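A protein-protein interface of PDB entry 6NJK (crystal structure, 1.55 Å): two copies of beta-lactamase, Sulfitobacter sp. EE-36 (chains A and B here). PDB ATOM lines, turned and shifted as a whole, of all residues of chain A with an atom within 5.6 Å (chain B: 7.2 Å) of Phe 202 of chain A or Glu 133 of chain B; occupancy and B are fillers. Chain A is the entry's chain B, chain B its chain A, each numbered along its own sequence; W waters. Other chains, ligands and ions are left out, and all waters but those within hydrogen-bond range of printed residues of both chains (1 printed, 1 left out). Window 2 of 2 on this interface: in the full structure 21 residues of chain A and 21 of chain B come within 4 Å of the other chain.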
ATOM      1  N   ALA A  49     -13.975 -17.646  -2.645  1.00  0.00           N
ATOM      2  CA  ALA A  49     -15.098 -16.727  -2.759  1.00  0.00           C
ATOM      3  C   ALA A  49     -16.429 -17.454  -2.648  1.00  0.00           C
ATOM      4  O   ALA A  49     -17.410 -16.892  -2.143  1.00  0.00           O
ATOM      5  CB  ALA A  49     -15.015 -16.007  -4.102  1.00  0.00           C
ATOM      6  N   ALA A  50     -16.481 -18.691  -3.131  1.00  0.00           N
ATOM      7  CA  ALA A  50     -17.694 -19.494  -3.132  1.00  0.00           C
ATOM      8  C   ALA A  50     -17.323 -20.935  -2.824  1.00  0.00           C
ATOM      9  O   ALA A  50     -16.423 -21.496  -3.457  1.00  0.00           O
ATOM     10  CB  ALA A  50     -18.409 -19.405  -4.484  1.00  0.00           C
ATOM     11  N   MET A 197     -21.121 -11.174 -11.947  1.00  0.00           N
ATOM     12  CA  MET A 197     -21.548 -12.189 -10.997  1.00  0.00           C
ATOM     13  C   MET A 197     -20.529 -13.305 -10.782  1.00  0.00           C
ATOM     14  O   MET A 197     -20.429 -13.837  -9.676  1.00  0.00           O
ATOM     15  CB  MET A 197     -22.877 -12.803 -11.459  1.00  0.00           C
ATOM     16  CG  MET A 197     -24.064 -11.884 -11.316  1.00  0.00           C
ATOM     17  SD  MET A 197     -24.659 -11.778  -9.465  1.00  0.00           S
ATOM     18  CE  MET A 197     -25.512 -10.023  -9.544  1.00  0.00           C
ATOM     19  N   TYR A 200     -18.515 -12.421  -7.823  1.00  0.00           N
ATOM     20  CA  TYR A 200     -19.200 -11.932  -6.628  1.00  0.00           C
ATOM     21  C   TYR A 200     -19.192 -13.040  -5.583  1.00  0.00           C
ATOM     22  O   TYR A 200     -19.866 -14.065  -5.740  1.00  0.00           O
ATOM     23  CB  TYR A 200     -20.616 -11.494  -6.986  1.00  0.00           C
ATOM     24  CG  TYR A 200     -21.382 -10.665  -5.971  1.00  0.00           C
ATOM     25  CD1 TYR A 200     -20.778 -10.109  -4.841  1.00  0.00           C
ATOM     26  CD2 TYR A 200     -22.732 -10.433  -6.163  1.00  0.00           C
ATOM     27  CE1 TYR A 200     -21.528  -9.345  -3.930  1.00  0.00           C
ATOM     28  CE2 TYR A 200     -23.471  -9.693  -5.281  1.00  0.00           C
ATOM     29  CZ  TYR A 200     -22.878  -9.145  -4.167  1.00  0.00           C
ATOM     30  OH  TYR A 200     -23.669  -8.408  -3.311  1.00  0.00           O
ATOM     31  N   ALA A 201     -18.424 -12.833  -4.519  1.00  0.00           N
ATOM     32  CA  ALA A 201     -18.339 -13.812  -3.451  1.00  0.00           C
ATOM     33  C   ALA A 201     -19.680 -13.983  -2.754  1.00  0.00           C
ATOM     34  O   ALA A 201     -20.509 -13.072  -2.714  1.00  0.00           O
ATOM     35  CB  ALA A 201     -17.298 -13.384  -2.418  1.00  0.00           C
ATOM     36  N   PHE A 202     -19.881 -15.163  -2.188  1.00  0.00           N
ATOM     37  CA  PHE A 202     -20.981 -15.382  -1.265  1.00  0.00           C
ATOM     38  C   PHE A 202     -20.479 -15.160   0.152  1.00  0.00           C
ATOM     39  O   PHE A 202     -19.316 -15.407   0.468  1.00  0.00           O
ATOM     40  CB  PHE A 202     -21.556 -16.782  -1.439  1.00  0.00           C
ATOM     41  CG  PHE A 202     -22.278 -16.961  -2.740  1.00  0.00           C
ATOM     42  CD1 PHE A 202     -23.575 -16.499  -2.900  1.00  0.00           C
ATOM     43  CD2 PHE A 202     -21.648 -17.549  -3.819  1.00  0.00           C
ATOM     44  CE1 PHE A 202     -24.239 -16.645  -4.112  1.00  0.00           C
ATOM     45  CE2 PHE A 202     -22.307 -17.702  -5.031  1.00  0.00           C
ATOM     46  CZ  PHE A 202     -23.601 -17.248  -5.178  1.00  0.00           C
ATOM     47  N   GLY A 203     -21.354 -14.633   0.997  1.00  0.00           N
ATOM     48  CA  GLY A 203     -21.080 -14.497   2.413  1.00  0.00           C
ATOM     49  C   GLY A 203     -21.678 -15.688   3.137  1.00  0.00           C
ATOM     50  O   GLY A 203     -22.663 -16.266   2.688  1.00  0.00           O
ATOM     51  N   TYR A 204     -21.073 -16.066   4.255  1.00  0.00           N
ATOM     52  CA  TYR A 204     -21.454 -17.296   4.943  1.00  0.00           C
ATOM     53  C   TYR A 204     -21.879 -16.976   6.367  1.00  0.00           C
ATOM     54  O   TYR A 204     -21.073 -16.512   7.180  1.00  0.00           O
ATOM     55  CB  TYR A 204     -20.316 -18.308   4.873  1.00  0.00           C
ATOM     56  CG  TYR A 204     -20.162 -18.806   3.456  1.00  0.00           C
ATOM     57  CD1 TYR A 204     -20.971 -19.823   2.971  1.00  0.00           C
ATOM     58  CD2 TYR A 204     -19.249 -18.226   2.589  1.00  0.00           C
ATOM     59  CE1 TYR A 204     -20.855 -20.267   1.677  1.00  0.00           C
ATOM     60  CE2 TYR A 204     -19.124 -18.663   1.293  1.00  0.00           C
ATOM     61  CZ  TYR A 204     -19.931 -19.683   0.841  1.00  0.00           C
ATOM     62  OH  TYR A 204     -19.820 -20.130  -0.454  1.00  0.00           O
ATOM     63  N   PRO A 211     -24.917 -19.735   2.547  1.00  0.00           N
ATOM     64  CA  PRO A 211     -24.638 -18.534   1.749  1.00  0.00           C
ATOM     65  C   PRO A 211     -25.747 -17.513   1.950  1.00  0.00           C
ATOM     66  O   PRO A 211     -26.934 -17.835   1.856  1.00  0.00           O
ATOM     67  CB  PRO A 211     -24.593 -19.053   0.306  1.00  0.00           C
ATOM     68  CG  PRO A 211     -24.569 -20.562   0.411  1.00  0.00           C
ATOM     69  CD  PRO A 211     -25.255 -20.893   1.700  1.00  0.00           C
ATOM     70  N   ILE A 212     -25.356 -16.276   2.238  1.00  0.00           N
ATOM     71  CA  ILE A 212     -26.316 -15.218   2.528  1.00  0.00           C
ATOM     72  C   ILE A 212     -25.858 -13.939   1.840  1.00  0.00           C
ATOM     73  O   ILE A 212     -24.664 -13.696   1.654  1.00  0.00           O
ATOM     74  CB  ILE A 212     -26.510 -15.038   4.056  1.00  0.00           C
ATOM     75  CG1 ILE A 212     -27.668 -14.074   4.344  1.00  0.00           C
ATOM     76  CG2 ILE A 212     -25.240 -14.553   4.730  1.00  0.00           C
ATOM     77  CD1 ILE A 212     -28.025 -13.936   5.822  1.00  0.00           C
ATOM     78  N   ARG A 213     -26.829 -13.136   1.431  1.00  0.00           N
ATOM     79  CA  ARG A 213     -26.608 -11.974   0.583  1.00  0.00           C
ATOM     80  C   ARG A 213     -27.288 -10.778   1.228  1.00  0.00           C
ATOM     81  O   ARG A 213     -28.405 -10.901   1.736  1.00  0.00           O
ATOM     82  CB  ARG A 213     -27.169 -12.254  -0.825  1.00  0.00           C
ATOM     83  CG  ARG A 213     -27.062 -11.140  -1.831  1.00  0.00           C
ATOM     84  CD  ARG A 213     -25.619 -10.844  -2.150  1.00  0.00           C
ATOM     85  NE  ARG A 213     -25.010 -11.840  -3.028  1.00  0.00           N
ATOM     86  CZ  ARG A 213     -23.734 -12.214  -2.967  1.00  0.00           C
ATOM     87  NH1 ARG A 213     -22.924 -11.700  -2.045  1.00  0.00           N
ATOM     88  NH2 ARG A 213     -23.273 -13.113  -3.823  1.00  0.00           N
ATOM     89  N   GLY A 323     -23.034 -11.655   6.109  1.00  0.00           N
ATOM     90  CA  GLY A 323     -22.154 -12.633   5.514  1.00  0.00           C
ATOM     91  C   GLY A 323     -20.711 -12.204   5.338  1.00  0.00           C
ATOM     92  O   GLY A 323     -19.893 -13.037   4.938  1.00  0.00           O
ATOM     93  N   PHE A 324     -20.370 -10.942   5.637  1.00  0.00           N
ATOM     94  CA  PHE A 324     -19.057 -10.398   5.311  1.00  0.00           C
ATOM     95  C   PHE A 324     -18.485  -9.575   6.459  1.00  0.00           C
ATOM     96  O   PHE A 324     -19.220  -8.963   7.239  1.00  0.00           O
ATOM     97  CB  PHE A 324     -19.108  -9.492   4.062  1.00  0.00           C
ATOM     98  CG  PHE A 324     -19.377 -10.225   2.780  1.00  0.00           C
ATOM     99  CD1 PHE A 324     -18.347 -10.501   1.903  1.00  0.00           C
ATOM    100  CD2 PHE A 324     -20.656 -10.623   2.444  1.00  0.00           C
ATOM    101  CE1 PHE A 324     -18.587 -11.168   0.726  1.00  0.00           C
ATOM    102  CE2 PHE A 324     -20.900 -11.288   1.262  1.00  0.00           C
ATOM    103  CZ  PHE A 324     -19.867 -11.559   0.402  1.00  0.00           C
ATOM    104  N   ASN A 343     -15.327 -13.086   3.521  1.00  0.00           N
ATOM    105  CA  ASN A 343     -16.725 -13.498   3.372  1.00  0.00           C
ATOM    106  C   ASN A 343     -17.205 -14.265   4.599  1.00  0.00           C
ATOM    107  O   ASN A 343     -17.928 -15.263   4.508  1.00  0.00           O
ATOM    108  CB  ASN A 343     -16.952 -14.298   2.087  1.00  0.00           C
ATOM    109  CG  ASN A 343     -16.093 -15.545   1.983  1.00  0.00           C
ATOM    110  OD1 ASN A 343     -15.291 -15.842   2.861  1.00  0.00           O
ATOM    111  ND2 ASN A 343     -16.268 -16.286   0.891  1.00  0.00           N
ATOM    112  N   GLY B 126     -32.554 -16.388   0.113  1.00  0.00           N
ATOM    113  CA  GLY B 126     -31.700 -15.489   0.865  1.00  0.00           C
ATOM    114  C   GLY B 126     -30.343 -15.243   0.242  1.00  0.00           C
ATOM    115  O   GLY B 126     -29.723 -14.211   0.521  1.00  0.00           O
ATOM    116  N   GLU B 127     -29.863 -16.169  -0.585  1.00  0.00           N
ATOM    117  CA  GLU B 127     -28.581 -16.017  -1.260  1.00  0.00           C
ATOM    118  C   GLU B 127     -28.686 -15.171  -2.526  1.00  0.00           C
ATOM    119  O   GLU B 127     -27.688 -15.027  -3.245  1.00  0.00           O
ATOM    120  CB  GLU B 127     -27.994 -17.398  -1.583  1.00  0.00           C
ATOM    121  CG  GLU B 127     -28.755 -18.217  -2.621  1.00  0.00           C
ATOM    122  CD  GLU B 127     -29.757 -19.195  -2.010  1.00  0.00           C
ATOM    123  OE1 GLU B 127     -30.370 -18.862  -0.973  1.00  0.00           O
ATOM    124  OE2 GLU B 127     -29.928 -20.303  -2.570  1.00  0.00           O
ATOM    125  N   VAL B 128     -29.864 -14.603  -2.788  1.00  0.00           N
ATOM    126  CA  VAL B 128     -30.127 -13.775  -3.960  1.00  0.00           C
ATOM    127  C   VAL B 128     -30.347 -12.339  -3.502  1.00  0.00           C
ATOM    128  O   VAL B 128     -31.191 -12.076  -2.635  1.00  0.00           O
ATOM    129  CB  VAL B 128     -31.341 -14.295  -4.750  1.00  0.00           C
ATOM    130  CG1 VAL B 128     -31.756 -13.276  -5.785  1.00  0.00           C
ATOM    131  CG2 VAL B 128     -31.008 -15.632  -5.393  1.00  0.00           C
ATOM    132  N   GLY B 129     -29.604 -11.408  -4.097  1.00  0.00           N
ATOM    133  CA  GLY B 129     -29.601 -10.041  -3.617  1.00  0.00           C
ATOM    134  C   GLY B 129     -30.177  -9.013  -4.570  1.00  0.00           C
ATOM    135  O   GLY B 129     -30.357  -7.851  -4.192  1.00  0.00           O
ATOM    136  N   ASN B 130     -30.448  -9.418  -5.809  1.00  0.00           N
ATOM    137  CA  ASN B 130     -31.080  -8.549  -6.794  1.00  0.00           C
ATOM    138  C   ASN B 130     -31.581  -9.424  -7.937  1.00  0.00           C
ATOM    139  O   ASN B 130     -31.366 -10.639  -7.957  1.00  0.00           O
ATOM    140  CB  ASN B 130     -30.127  -7.433  -7.284  1.00  0.00           C
ATOM    141  CG  ASN B 130     -28.869  -7.950  -7.990  1.00  0.00           C
ATOM    142  OD1 ASN B 130     -28.700  -9.148  -8.219  1.00  0.00           O
ATOM    143  ND2 ASN B 130     -27.977  -7.023  -8.346  1.00  0.00           N
ATOM    144  N   VAL B 131     -32.285  -8.797  -8.881  1.00  0.00           N
ATOM    145  CA  VAL B 131     -32.881  -9.588  -9.955  1.00  0.00           C
ATOM    146  C   VAL B 131     -31.804 -10.230 -10.829  1.00  0.00           C
ATOM    147  O   VAL B 131     -31.985 -11.349 -11.327  1.00  0.00           O
ATOM    148  CB  VAL B 131     -33.845  -8.732 -10.791  1.00  0.00           C
ATOM    149  CG1 VAL B 131     -34.317  -9.512 -12.000  1.00  0.00           C
ATOM    150  CG2 VAL B 131     -35.040  -8.316  -9.956  1.00  0.00           C
ATOM    151  N   ALA B 132     -30.667  -9.562 -11.027  1.00  0.00           N
ATOM    152  CA  ALA B 132     -29.611 -10.174 -11.829  1.00  0.00           C
ATOM    153  C   ALA B 132     -29.147 -11.492 -11.212  1.00  0.00           C
ATOM    154  O   ALA B 132     -28.972 -12.490 -11.922  1.00  0.00           O
ATOM    155  CB  ALA B 132     -28.440  -9.207 -11.991  1.00  0.00           C
ATOM    156  N   GLU B 133     -28.946 -11.518  -9.890  1.00  0.00           N
ATOM    157  CA  GLU B 133     -28.534 -12.748  -9.220  1.00  0.00           C
ATOM    158  C   GLU B 133     -29.656 -13.778  -9.226  1.00  0.00           C
ATOM    159  O   GLU B 133     -29.390 -14.986  -9.272  1.00  0.00           O
ATOM    160  CB  GLU B 133     -28.086 -12.436  -7.791  1.00  0.00           C
ATOM    161  CG  GLU B 133     -27.333 -13.568  -7.107  1.00  0.00           C
ATOM    162  CD  GLU B 133     -26.529 -13.098  -5.906  1.00  0.00           C
ATOM    163  OE1 GLU B 133     -27.030 -12.230  -5.156  1.00  0.00           O
ATOM    164  OE2 GLU B 133     -25.388 -13.589  -5.727  1.00  0.00           O
ATOM    165  N   LEU B 134     -30.909 -13.319  -9.191  1.00  0.00           N
ATOM    166  CA  LEU B 134     -32.039 -14.235  -9.277  1.00  0.00           C
ATOM    167  C   LEU B 134     -32.039 -14.971 -10.606  1.00  0.00           C
ATOM    168  O   LEU B 134     -32.242 -16.188 -10.657  1.00  0.00           O
ATOM    169  CB  LEU B 134     -33.351 -13.476  -9.100  1.00  0.00           C
ATOM    170  CG  LEU B 134     -34.593 -14.362  -9.219  1.00  0.00           C
ATOM    171  CD1 LEU B 134     -34.575 -15.436  -8.159  1.00  0.00           C
ATOM    172  CD2 LEU B 134     -35.846 -13.518  -9.106  1.00  0.00           C
ATOM    173  N   ILE B 135     -31.823 -14.243 -11.701  1.00  0.00           N
ATOM    174  CA  ILE B 135     -31.762 -14.886 -13.007  1.00  0.00           C
ATOM    175  C   ILE B 135     -30.627 -15.903 -13.038  1.00  0.00           C
ATOM    176  O   ILE B 135     -30.766 -16.992 -13.606  1.00  0.00           O
ATOM    177  CB  ILE B 135     -31.640 -13.819 -14.112  1.00  0.00           C
ATOM    178  CG1 ILE B 135     -32.943 -13.010 -14.180  1.00  0.00           C
ATOM    179  CG2 ILE B 135     -31.317 -14.468 -15.437  1.00  0.00           C
ATOM    180  CD1 ILE B 135     -32.826 -11.687 -14.915  1.00  0.00           C
ATOM    181  N   ARG B 136     -29.503 -15.589 -12.390  1.00  0.00           N
ATOM    182  CA  ARG B 136     -28.386 -16.530 -12.335  1.00  0.00           C
ATOM    183  C   ARG B 136     -28.754 -17.784 -11.548  1.00  0.00           C
ATOM    184  O   ARG B 136     -28.392 -18.899 -11.943  1.00  0.00           O
ATOM    185  CB  ARG B 136     -27.175 -15.827 -11.725  1.00  0.00           C
ATOM    186  CG  ARG B 136     -25.920 -16.661 -11.566  1.00  0.00           C
ATOM    187  CD  ARG B 136     -24.813 -15.776 -10.990  1.00  0.00           C
ATOM    188  NE  ARG B 136     -23.560 -16.491 -10.768  1.00  0.00           N
ATOM    189  CZ  ARG B 136     -22.610 -16.645 -11.686  1.00  0.00           C
ATOM    190  NH1 ARG B 136     -22.766 -16.144 -12.905  1.00  0.00           N
ATOM    191  NH2 ARG B 136     -21.504 -17.310 -11.384  1.00  0.00           N
ATOM    192  N   TRP B 137     -29.472 -17.620 -10.435  1.00  0.00           N
ATOM    193  CA  TRP B 137     -29.946 -18.759  -9.658  1.00  0.00           C
ATOM    194  C   TRP B 137     -30.892 -19.622 -10.475  1.00  0.00           C
ATOM    195  O   TRP B 137     -30.826 -20.857 -10.422  1.00  0.00           O
ATOM    196  CB  TRP B 137     -30.625 -18.205  -8.407  1.00  0.00           C
ATOM    197  CG  TRP B 137     -31.046 -19.164  -7.360  1.00  0.00           C
ATOM    198  CD1 TRP B 137     -30.320 -19.561  -6.280  1.00  0.00           C
ATOM    199  CD2 TRP B 137     -32.316 -19.815  -7.255  1.00  0.00           C
ATOM    200  NE1 TRP B 137     -31.052 -20.433  -5.514  1.00  0.00           N
ATOM    201  CE2 TRP B 137     -32.284 -20.603  -6.090  1.00  0.00           C
ATOM    202  CE3 TRP B 137     -33.477 -19.808  -8.031  1.00  0.00           C
ATOM    203  CZ2 TRP B 137     -33.363 -21.385  -5.687  1.00  0.00           C
ATOM    204  CZ3 TRP B 137     -34.548 -20.586  -7.628  1.00  0.00           C
ATOM    205  CH2 TRP B 137     -34.482 -21.365  -6.470  1.00  0.00           C
ATOM    206  N   LEU B 138     -31.755 -18.991 -11.266  1.00  0.00           N
ATOM    207  CA  LEU B 138     -32.733 -19.736 -12.043  1.00  0.00           C
ATOM    208  C   LEU B 138     -32.094 -20.565 -13.148  1.00  0.00           C
ATOM    209  O   LEU B 138     -32.722 -21.515 -13.636  1.00  0.00           O
ATOM    210  CB  LEU B 138     -33.755 -18.766 -12.630  1.00  0.00           C
ATOM    211  CG  LEU B 138     -34.733 -18.194 -11.606  1.00  0.00           C
ATOM    212  CD1 LEU B 138     -35.531 -17.034 -12.186  1.00  0.00           C
ATOM    213  CD2 LEU B 138     -35.662 -19.287 -11.086  1.00  0.00           C
ATOM    214  N   GLU B 139     -30.864 -20.235 -13.555  1.00  0.00           N
ATOM    215  CA  GLU B 139     -30.198 -21.013 -14.593  1.00  0.00           C
ATOM    216  C   GLU B 139     -30.093 -22.483 -14.206  1.00  0.00           C
ATOM    217  O   GLU B 139     -30.169 -23.361 -15.073  1.00  0.00           O
ATOM    218  CB  GLU B 139     -28.802 -20.446 -14.874  1.00  0.00           C
ATOM    219  CG  GLU B 139     -28.790 -19.068 -15.530  1.00  0.00           C
ATOM    220  CD  GLU B 139     -27.385 -18.476 -15.658  1.00  0.00           C
ATOM    221  OE1 GLU B 139     -26.395 -19.190 -15.387  1.00  0.00           O
ATOM    222  OE2 GLU B 139     -27.270 -17.288 -16.032  1.00  0.00           O
HETATM  223  O   HOH W   1     -28.705 -19.576   1.701  1.00  0.00           O
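Asn 130 of chain B touches Met 197 of chain A (OD1 to CE, 3.6 Å). Met 197 of chain A touches Ala 132 of chain B (CE to CB, 3.9 Å). Met 197 of chain A touches Glu 133 of chain B. CD of Arg 136 of chain B touches CB of Met 197 of chain A, 3.6 Å away. Glu 127 of chain B touches Phe 202 of chain A (O to CE1, 3.9 Å). CE1 of Phe 202 of chain A touches OE2 of Glu 133 of chain B, 3.6 Å away. O of Pro 211 of chain A touches CB of Glu 127 of chain B (3.6 Å). Glu 127 of chain B touches Arg 213 of chain A (C to CB, 3.7 Å). Val 128 of chain B touches Arg 213 of chain A. Gly 129 of chain B touches Arg 213 of chain A.
The backbone NH of Arg 213 of chain A is in hydrogen-bond range of the backbone carbonyl oxygen of Gly 126 of chain B, 3.2 Å away. NH2 of Arg 213 of chain A is in salt-bridge range of OE2 of Glu 133 of chain B (2.9 Å).
Printed residues of chain B within 4 Å of Met 197 of chain A: Asn 130 (3.6 Å), Ala 132 (3.9 Å), Glu 133 (3.8 Å) and Arg 136 (3.6 Å). Of chain B, only Glu 127 (3.9 Å) and Glu 133 (3.6 Å) come within 4 Å of Phe 202 of chain A. Of the printed residues of chain B, Pro 211 of chain A touches Glu 127. Of the printed residues of chain A, Val 128 of chain B touches Arg 213. Printed residues of chain A within 4 Å of Asn 130 of chain B: Met 197. Of the printed residues of chain A, Ala 132 of chain B touches Met 197. Of chain A, only Met 197, Phe 202 and Arg 213 come within 4 Å of Glu 133 of chain B. The nearest printed residue of chain A that does not touch Glu 127 of chain B is Ile 212 of chain A (4.5 Å).
Water W1 lies within hydrogen-bond range of O of Pro 211 of chain A and OE1 of Glu 127 of chain B.
The side-chain carboxylate (OE2) of Glu 127 of chain B sits at hydrogen-bond distance from the indole nitrogen (NE1) of Trp 137 of chain B (3.2 Å). The side-chain carboxylate (OE1) of Glu 133 of chain B lies within hydrogen-bond range of the backbone NH (N) of Gly 129 of chain B, at 2.9 Å. The side-chain amide oxygen (OD1) of Asn 130 of chain B lies close to the backbone NH (N) of Ala 132 of chain B (3.5 Å). The backbone NH (N) of Glu 133 of chain B lies within hydrogen-bond range of the side-chain amide oxygen (OD1) of Asn 130 of chain B (2.9 Å). N of Phe 202 of chain A sits at hydrogen-bond distance from O of Ala 49 of chain A (3.0 Å). O of Ala 201 of chain A sits at hydrogen-bond distance from NH1 of Arg 213 of chain A, 2.9 Å away.
No position is printed for both chains. Of the 12 pairs that touch across the chains among the printed residues, none has its exchanged pair printed and touching as well.
Of the 14 printed residues of chain A, 4 touch a printed residue of chain B. Hydrophobic or aromatic side chains of chain B within 4 Å of the printed part of chain A: Ala 132. Among the printed residues, 12 pairs touch across the chains. Among the printed residues, Asp or Glu carboxylates within 4 Å of a Lys or Arg side-chain nitrogen of the other chain: Arg 213 of chain A with Glu 133 of chain B (2.9 Å).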
